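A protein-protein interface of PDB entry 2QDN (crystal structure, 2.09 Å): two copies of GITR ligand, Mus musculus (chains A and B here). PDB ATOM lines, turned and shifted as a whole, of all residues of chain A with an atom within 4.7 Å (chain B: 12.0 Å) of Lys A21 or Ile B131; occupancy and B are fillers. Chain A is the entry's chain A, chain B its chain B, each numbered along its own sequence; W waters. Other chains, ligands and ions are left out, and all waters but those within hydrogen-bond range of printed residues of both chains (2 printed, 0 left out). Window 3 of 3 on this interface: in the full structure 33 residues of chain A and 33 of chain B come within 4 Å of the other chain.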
ATOM      1  N   LYS A  14      -6.990 -19.249   3.755  1.00  0.00           N
ATOM      2  CA  LYS A  14      -7.548 -20.584   3.780  1.00  0.00           C
ATOM      3  C   LYS A  14      -7.007 -21.405   2.618  1.00  0.00           C
ATOM      4  O   LYS A  14      -7.123 -21.001   1.456  1.00  0.00           O
ATOM      5  CB  LYS A  14      -9.074 -20.528   3.713  1.00  0.00           C
ATOM      6  CG  LYS A  14      -9.704 -21.914   3.924  1.00  0.00           C
ATOM      7  CD  LYS A  14     -11.093 -22.006   3.313  1.00  0.00           C
ATOM      8  CE  LYS A  14     -12.142 -21.563   4.282  1.00  0.00           C
ATOM      9  NZ  LYS A  14     -13.471 -22.110   3.869  1.00  0.00           N
ATOM     10  N   PHE A  15      -6.423 -22.555   2.940  1.00  0.00           N
ATOM     11  CA  PHE A  15      -5.847 -23.448   1.946  1.00  0.00           C
ATOM     12  C   PHE A  15      -6.811 -24.583   1.665  1.00  0.00           C
ATOM     13  O   PHE A  15      -7.254 -25.240   2.597  1.00  0.00           O
ATOM     14  CB  PHE A  15      -4.523 -24.038   2.441  1.00  0.00           C
ATOM     15  CG  PHE A  15      -3.832 -24.902   1.440  1.00  0.00           C
ATOM     16  CD1 PHE A  15      -3.217 -24.340   0.330  1.00  0.00           C
ATOM     17  CD2 PHE A  15      -3.796 -26.292   1.614  1.00  0.00           C
ATOM     18  CE1 PHE A  15      -2.544 -25.164  -0.610  1.00  0.00           C
ATOM     19  CE2 PHE A  15      -3.144 -27.123   0.698  1.00  0.00           C
ATOM     20  CZ  PHE A  15      -2.518 -26.560  -0.411  1.00  0.00           C
ATOM     21  N   GLU A  16      -7.129 -24.796   0.387  1.00  0.00           N
ATOM     22  CA  GLU A  16      -8.057 -25.849  -0.016  1.00  0.00           C
ATOM     23  C   GLU A  16      -7.222 -26.910  -0.648  1.00  0.00           C
ATOM     24  O   GLU A  16      -6.649 -26.683  -1.706  1.00  0.00           O
ATOM     25  CB  GLU A  16      -9.069 -25.348  -1.056  1.00  0.00           C
ATOM     26  CG  GLU A  16     -10.048 -24.313  -0.554  1.00  0.00           C
ATOM     27  CD  GLU A  16     -11.169 -24.895   0.287  1.00  0.00           C
ATOM     28  OE1 GLU A  16     -11.299 -26.144   0.392  1.00  0.00           O
ATOM     29  OE2 GLU A  16     -11.928 -24.090   0.850  1.00  0.00           O
ATOM     30  N   SER A  19      -7.586 -28.172  -4.470  1.00  0.00           N
ATOM     31  CA  SER A  19      -7.102 -27.334  -5.575  1.00  0.00           C
ATOM     32  C   SER A  19      -5.685 -26.844  -5.348  1.00  0.00           C
ATOM     33  O   SER A  19      -5.075 -26.261  -6.240  1.00  0.00           O
ATOM     34  CB  SER A  19      -8.019 -26.109  -5.722  1.00  0.00           C
ATOM     35  OG  SER A  19      -8.020 -25.335  -4.518  1.00  0.00           O
ATOM     36  N   SER A  20      -5.172 -27.048  -4.131  1.00  0.00           N
ATOM     37  CA  SER A  20      -3.908 -26.460  -3.690  1.00  0.00           C
ATOM     38  C   SER A  20      -3.849 -24.950  -3.877  1.00  0.00           C
ATOM     39  O   SER A  20      -2.789 -24.404  -4.138  1.00  0.00           O
ATOM     40  CB  SER A  20      -2.709 -27.139  -4.344  1.00  0.00           C
ATOM     41  OG  SER A  20      -2.453 -28.398  -3.727  1.00  0.00           O
ATOM     42  N   LYS A  21      -4.997 -24.289  -3.702  1.00  0.00           N
ATOM     43  CA  LYS A  21      -5.089 -22.826  -3.682  1.00  0.00           C
ATOM     44  C   LYS A  21      -5.342 -22.276  -2.268  1.00  0.00           C
ATOM     45  O   LYS A  21      -6.090 -22.870  -1.488  1.00  0.00           O
ATOM     46  CB  LYS A  21      -6.220 -22.316  -4.587  1.00  0.00           C
ATOM     47  CG  LYS A  21      -6.198 -22.849  -6.014  1.00  0.00           C
ATOM     48  CD  LYS A  21      -4.926 -22.447  -6.750  1.00  0.00           C
ATOM     49  CE  LYS A  21      -5.031 -22.787  -8.251  1.00  0.00           C
ATOM     50  NZ  LYS A  21      -3.872 -22.172  -8.974  1.00  0.00           N
ATOM     51  N   TRP A  22      -4.735 -21.126  -1.991  1.00  0.00           N
ATOM     52  CA  TRP A  22      -5.064 -20.272  -0.848  1.00  0.00           C
ATOM     53  C   TRP A  22      -6.125 -19.221  -1.205  1.00  0.00           C
ATOM     54  O   TRP A  22      -6.028 -18.548  -2.235  1.00  0.00           O
ATOM     55  CB  TRP A  22      -3.804 -19.551  -0.349  1.00  0.00           C
ATOM     56  CG  TRP A  22      -2.809 -20.435   0.306  1.00  0.00           C
ATOM     57  CD1 TRP A  22      -1.712 -20.997  -0.266  1.00  0.00           C
ATOM     58  CD2 TRP A  22      -2.788 -20.830   1.692  1.00  0.00           C
ATOM     59  NE1 TRP A  22      -1.005 -21.738   0.667  1.00  0.00           N
ATOM     60  CE2 TRP A  22      -1.642 -21.646   1.878  1.00  0.00           C
ATOM     61  CE3 TRP A  22      -3.633 -20.580   2.789  1.00  0.00           C
ATOM     62  CZ2 TRP A  22      -1.322 -22.228   3.106  1.00  0.00           C
ATOM     63  CZ3 TRP A  22      -3.312 -21.166   4.038  1.00  0.00           C
ATOM     64  CH2 TRP A  22      -2.161 -21.979   4.175  1.00  0.00           C
ATOM     65  N   HIS A  23      -7.126 -19.092  -0.342  1.00  0.00           N
ATOM     66  CA  HIS A  23      -8.098 -18.009  -0.398  1.00  0.00           C
ATOM     67  C   HIS A  23      -7.781 -17.007   0.707  1.00  0.00           C
ATOM     68  O   HIS A  23      -7.554 -17.399   1.857  1.00  0.00           O
ATOM     69  CB  HIS A  23      -9.514 -18.578  -0.301  1.00  0.00           C
ATOM     70  CG  HIS A  23      -9.807 -19.591  -1.368  1.00  0.00           C
ATOM     71  ND1 HIS A  23     -10.758 -19.393  -2.345  1.00  0.00           N
ATOM     72  CD2 HIS A  23      -9.233 -20.789  -1.640  1.00  0.00           C
ATOM     73  CE1 HIS A  23     -10.784 -20.441  -3.150  1.00  0.00           C
ATOM     74  NE2 HIS A  23      -9.865 -21.300  -2.745  1.00  0.00           N
ATOM     75  N   PRO B 126     -13.977 -12.536   7.589  1.00  0.00           N
ATOM     76  CA  PRO B 126     -14.004 -11.593   6.479  1.00  0.00           C
ATOM     77  C   PRO B 126     -14.161 -12.415   5.196  1.00  0.00           C
ATOM     78  O   PRO B 126     -13.967 -13.644   5.213  1.00  0.00           O
ATOM     79  CB  PRO B 126     -12.637 -10.932   6.556  1.00  0.00           C
ATOM     80  CG  PRO B 126     -11.741 -11.983   7.152  1.00  0.00           C
ATOM     81  CD  PRO B 126     -12.623 -12.728   8.136  1.00  0.00           C
ATOM     82  N   ASP B 127     -14.546 -11.752   4.109  1.00  0.00           N
ATOM     83  CA  ASP B 127     -14.549 -12.381   2.781  1.00  0.00           C
ATOM     84  C   ASP B 127     -13.127 -12.757   2.394  1.00  0.00           C
ATOM     85  O   ASP B 127     -12.176 -12.098   2.804  1.00  0.00           O
ATOM     86  CB  ASP B 127     -15.155 -11.431   1.747  1.00  0.00           C
ATOM     87  CG  ASP B 127     -16.618 -11.065   2.069  1.00  0.00           C
ATOM     88  OD1 ASP B 127     -17.421 -11.978   2.382  1.00  0.00           O
ATOM     89  OD2 ASP B 127     -16.958  -9.865   2.004  1.00  0.00           O
ATOM     90  N   LEU B 128     -12.983 -13.819   1.619  1.00  0.00           N
ATOM     91  CA  LEU B 128     -11.665 -14.272   1.164  1.00  0.00           C
ATOM     92  C   LEU B 128     -11.609 -14.225  -0.368  1.00  0.00           C
ATOM     93  O   LEU B 128     -11.529 -15.263  -1.025  1.00  0.00           O
ATOM     94  CB  LEU B 128     -11.347 -15.682   1.694  1.00  0.00           C
ATOM     95  CG  LEU B 128     -11.406 -15.900   3.212  1.00  0.00           C
ATOM     96  CD1 LEU B 128     -11.372 -17.393   3.616  1.00  0.00           C
ATOM     97  CD2 LEU B 128     -10.304 -15.108   3.908  1.00  0.00           C
ATOM     98  N   PRO B 129     -11.610 -13.007  -0.946  1.00  0.00           N
ATOM     99  CA  PRO B 129     -11.824 -12.947  -2.403  1.00  0.00           C
ATOM    100  C   PRO B 129     -10.573 -13.194  -3.274  1.00  0.00           C
ATOM    101  O   PRO B 129     -10.702 -13.333  -4.493  1.00  0.00           O
ATOM    102  CB  PRO B 129     -12.362 -11.528  -2.611  1.00  0.00           C
ATOM    103  CG  PRO B 129     -11.847 -10.728  -1.457  1.00  0.00           C
ATOM    104  CD  PRO B 129     -11.421 -11.664  -0.361  1.00  0.00           C
ATOM    105  N   PHE B 130      -9.389 -13.257  -2.658  1.00  0.00           N
ATOM    106  CA  PHE B 130      -8.150 -13.336  -3.414  1.00  0.00           C
ATOM    107  C   PHE B 130      -7.544 -14.726  -3.396  1.00  0.00           C
ATOM    108  O   PHE B 130      -7.183 -15.258  -2.339  1.00  0.00           O
ATOM    109  CB  PHE B 130      -7.150 -12.270  -2.948  1.00  0.00           C
ATOM    110  CG  PHE B 130      -7.663 -10.881  -3.131  1.00  0.00           C
ATOM    111  CD1 PHE B 130      -7.631 -10.274  -4.403  1.00  0.00           C
ATOM    112  CD2 PHE B 130      -8.225 -10.197  -2.069  1.00  0.00           C
ATOM    113  CE1 PHE B 130      -8.137  -8.985  -4.588  1.00  0.00           C
ATOM    114  CE2 PHE B 130      -8.731  -8.897  -2.243  1.00  0.00           C
ATOM    115  CZ  PHE B 130      -8.689  -8.298  -3.500  1.00  0.00           C
ATOM    116  N   ILE B 131      -7.464 -15.310  -4.584  1.00  0.00           N
ATOM    117  CA  ILE B 131      -7.081 -16.692  -4.731  1.00  0.00           C
ATOM    118  C   ILE B 131      -5.723 -16.777  -5.390  1.00  0.00           C
ATOM    119  O   ILE B 131      -5.474 -16.127  -6.392  1.00  0.00           O
ATOM    120  CB  ILE B 131      -8.134 -17.506  -5.553  1.00  0.00           C
ATOM    121  CG1 ILE B 131      -9.541 -17.332  -4.967  1.00  0.00           C
ATOM    122  CG2 ILE B 131      -7.771 -19.005  -5.627  1.00  0.00           C
ATOM    123  CD1 ILE B 131     -10.652 -17.684  -5.942  1.00  0.00           C
ATOM    124  N   SER B 132      -4.824 -17.494  -4.734  1.00  0.00           N
ATOM    125  CA  SER B 132      -3.818 -18.342  -5.379  1.00  0.00           C
ATOM    126  C   SER B 132      -2.890 -18.831  -4.324  1.00  0.00           C
ATOM    127  O   SER B 132      -2.931 -20.028  -4.002  1.00  0.00           O
ATOM    128  CB  SER B 132      -3.019 -17.679  -6.485  1.00  0.00           C
ATOM    129  OG  SER B 132      -2.369 -18.691  -7.247  1.00  0.00           O
ATOM    130  OXT SER B 132      -2.148 -17.988  -3.789  1.00  0.00           O
HETATM  131  O   HOH W   1      -1.396 -22.217  -4.073  1.00  0.00           O
HETATM  132  O   HOH W   2     -12.845 -17.479  -1.755  1.00  0.00           O
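Leu B128 touches Lys A14 (CD1 to CB, 3.9 Å).
Lys A21 touches Ile B131.
Ser B132 touches Lys A21 (O to CA, 3.5 Å).
Ile B131 touches Trp A22.
Leu B128 touches His A23.
CA of His A23 touches O of Phe B130, 3.5 Å away.
ND1 of His A23 touches CG1 of Ile B131, 3.6 Å away.
No position is printed for both chains.
Of the 9 pairs that touch across the chains among the printed residues, none has its exchanged pair printed and touching as well.
Of the 8 printed residues of chain A, 4 touch a printed residue of chain B.
Of the 7 printed residues of chain B, 4 touch a printed residue of chain A.
Hydrophobic or aromatic side chains of chain B within 4 Å of the printed part of chain A: Leu B128 and Ile B131.
Among the printed residues, 9 pairs touch across the chains.
The side-chain amino group (NZ) of Lys A14 is in salt-bridge range of the side-chain carboxylate (OE2) of Glu A16, at 3.9 Å.
O of Lys A21 lies within hydrogen-bond range of N of Glu A16 (2.9 Å).
The side-chain hydroxyl of Ser A19 lies close to the backbone NH of Lys A21 (3.3 Å).
The backbone carbonyl oxygen of Lys A14 sits at hydrogen-bond distance from the backbone NH of His A23 (2.6 Å).
Water W1 bridges the backbone carbonyl oxygen (O) of Ser A20 and the chain-end carboxylate (O) of Ser B132.
Water W2 bridges O of Leu B128 (2.7 Å) and ND1 of His A23 (2.9 Å).
The backbone NH of Trp A22 sits at hydrogen-bond distance from the chain-end carboxylate of Ser B132 (2.9 Å).
The backbone carbonyl oxygen of Phe B130 sits close to the backbone carbonyl oxygen of Trp A22, 3.5 Å away.
Of the printed residues of chain B, Lys A21 touches Ile B131 (3.8 Å) and Ser B132 (3.5 Å).
Printed residues of chain A within 4 Å of Ile B131: Lys A21 (3.8 Å), Trp A22 (3.3 Å) and His A23 (3.6 Å).
No residue of chain B comes within 4 Å of Glu A16.
No residue of chain B comes within 4 Å of Ser A19.
Of chain B, only Phe B130, Ile B131 and Ser B132 come within 4 Å of Trp A22.
Printed residues of chain A within 4 Å of Leu B128: Lys A14 (3.9 Å) and His A23 (3.9 Å).
Of the printed residues of chain A, Phe B130 touches Trp A22 (3.5 Å) and His A23 (3.5 Å).
Printed residues of chain B within 4 Å of Lys A14: Leu B128.
The nearest printed residue of chain A that does not touch Ile B131 is Ser A19 (6.4 Å).
The nearest printed residue of chain A that does not touch Leu B128 is Trp A22 (6.5 Å).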
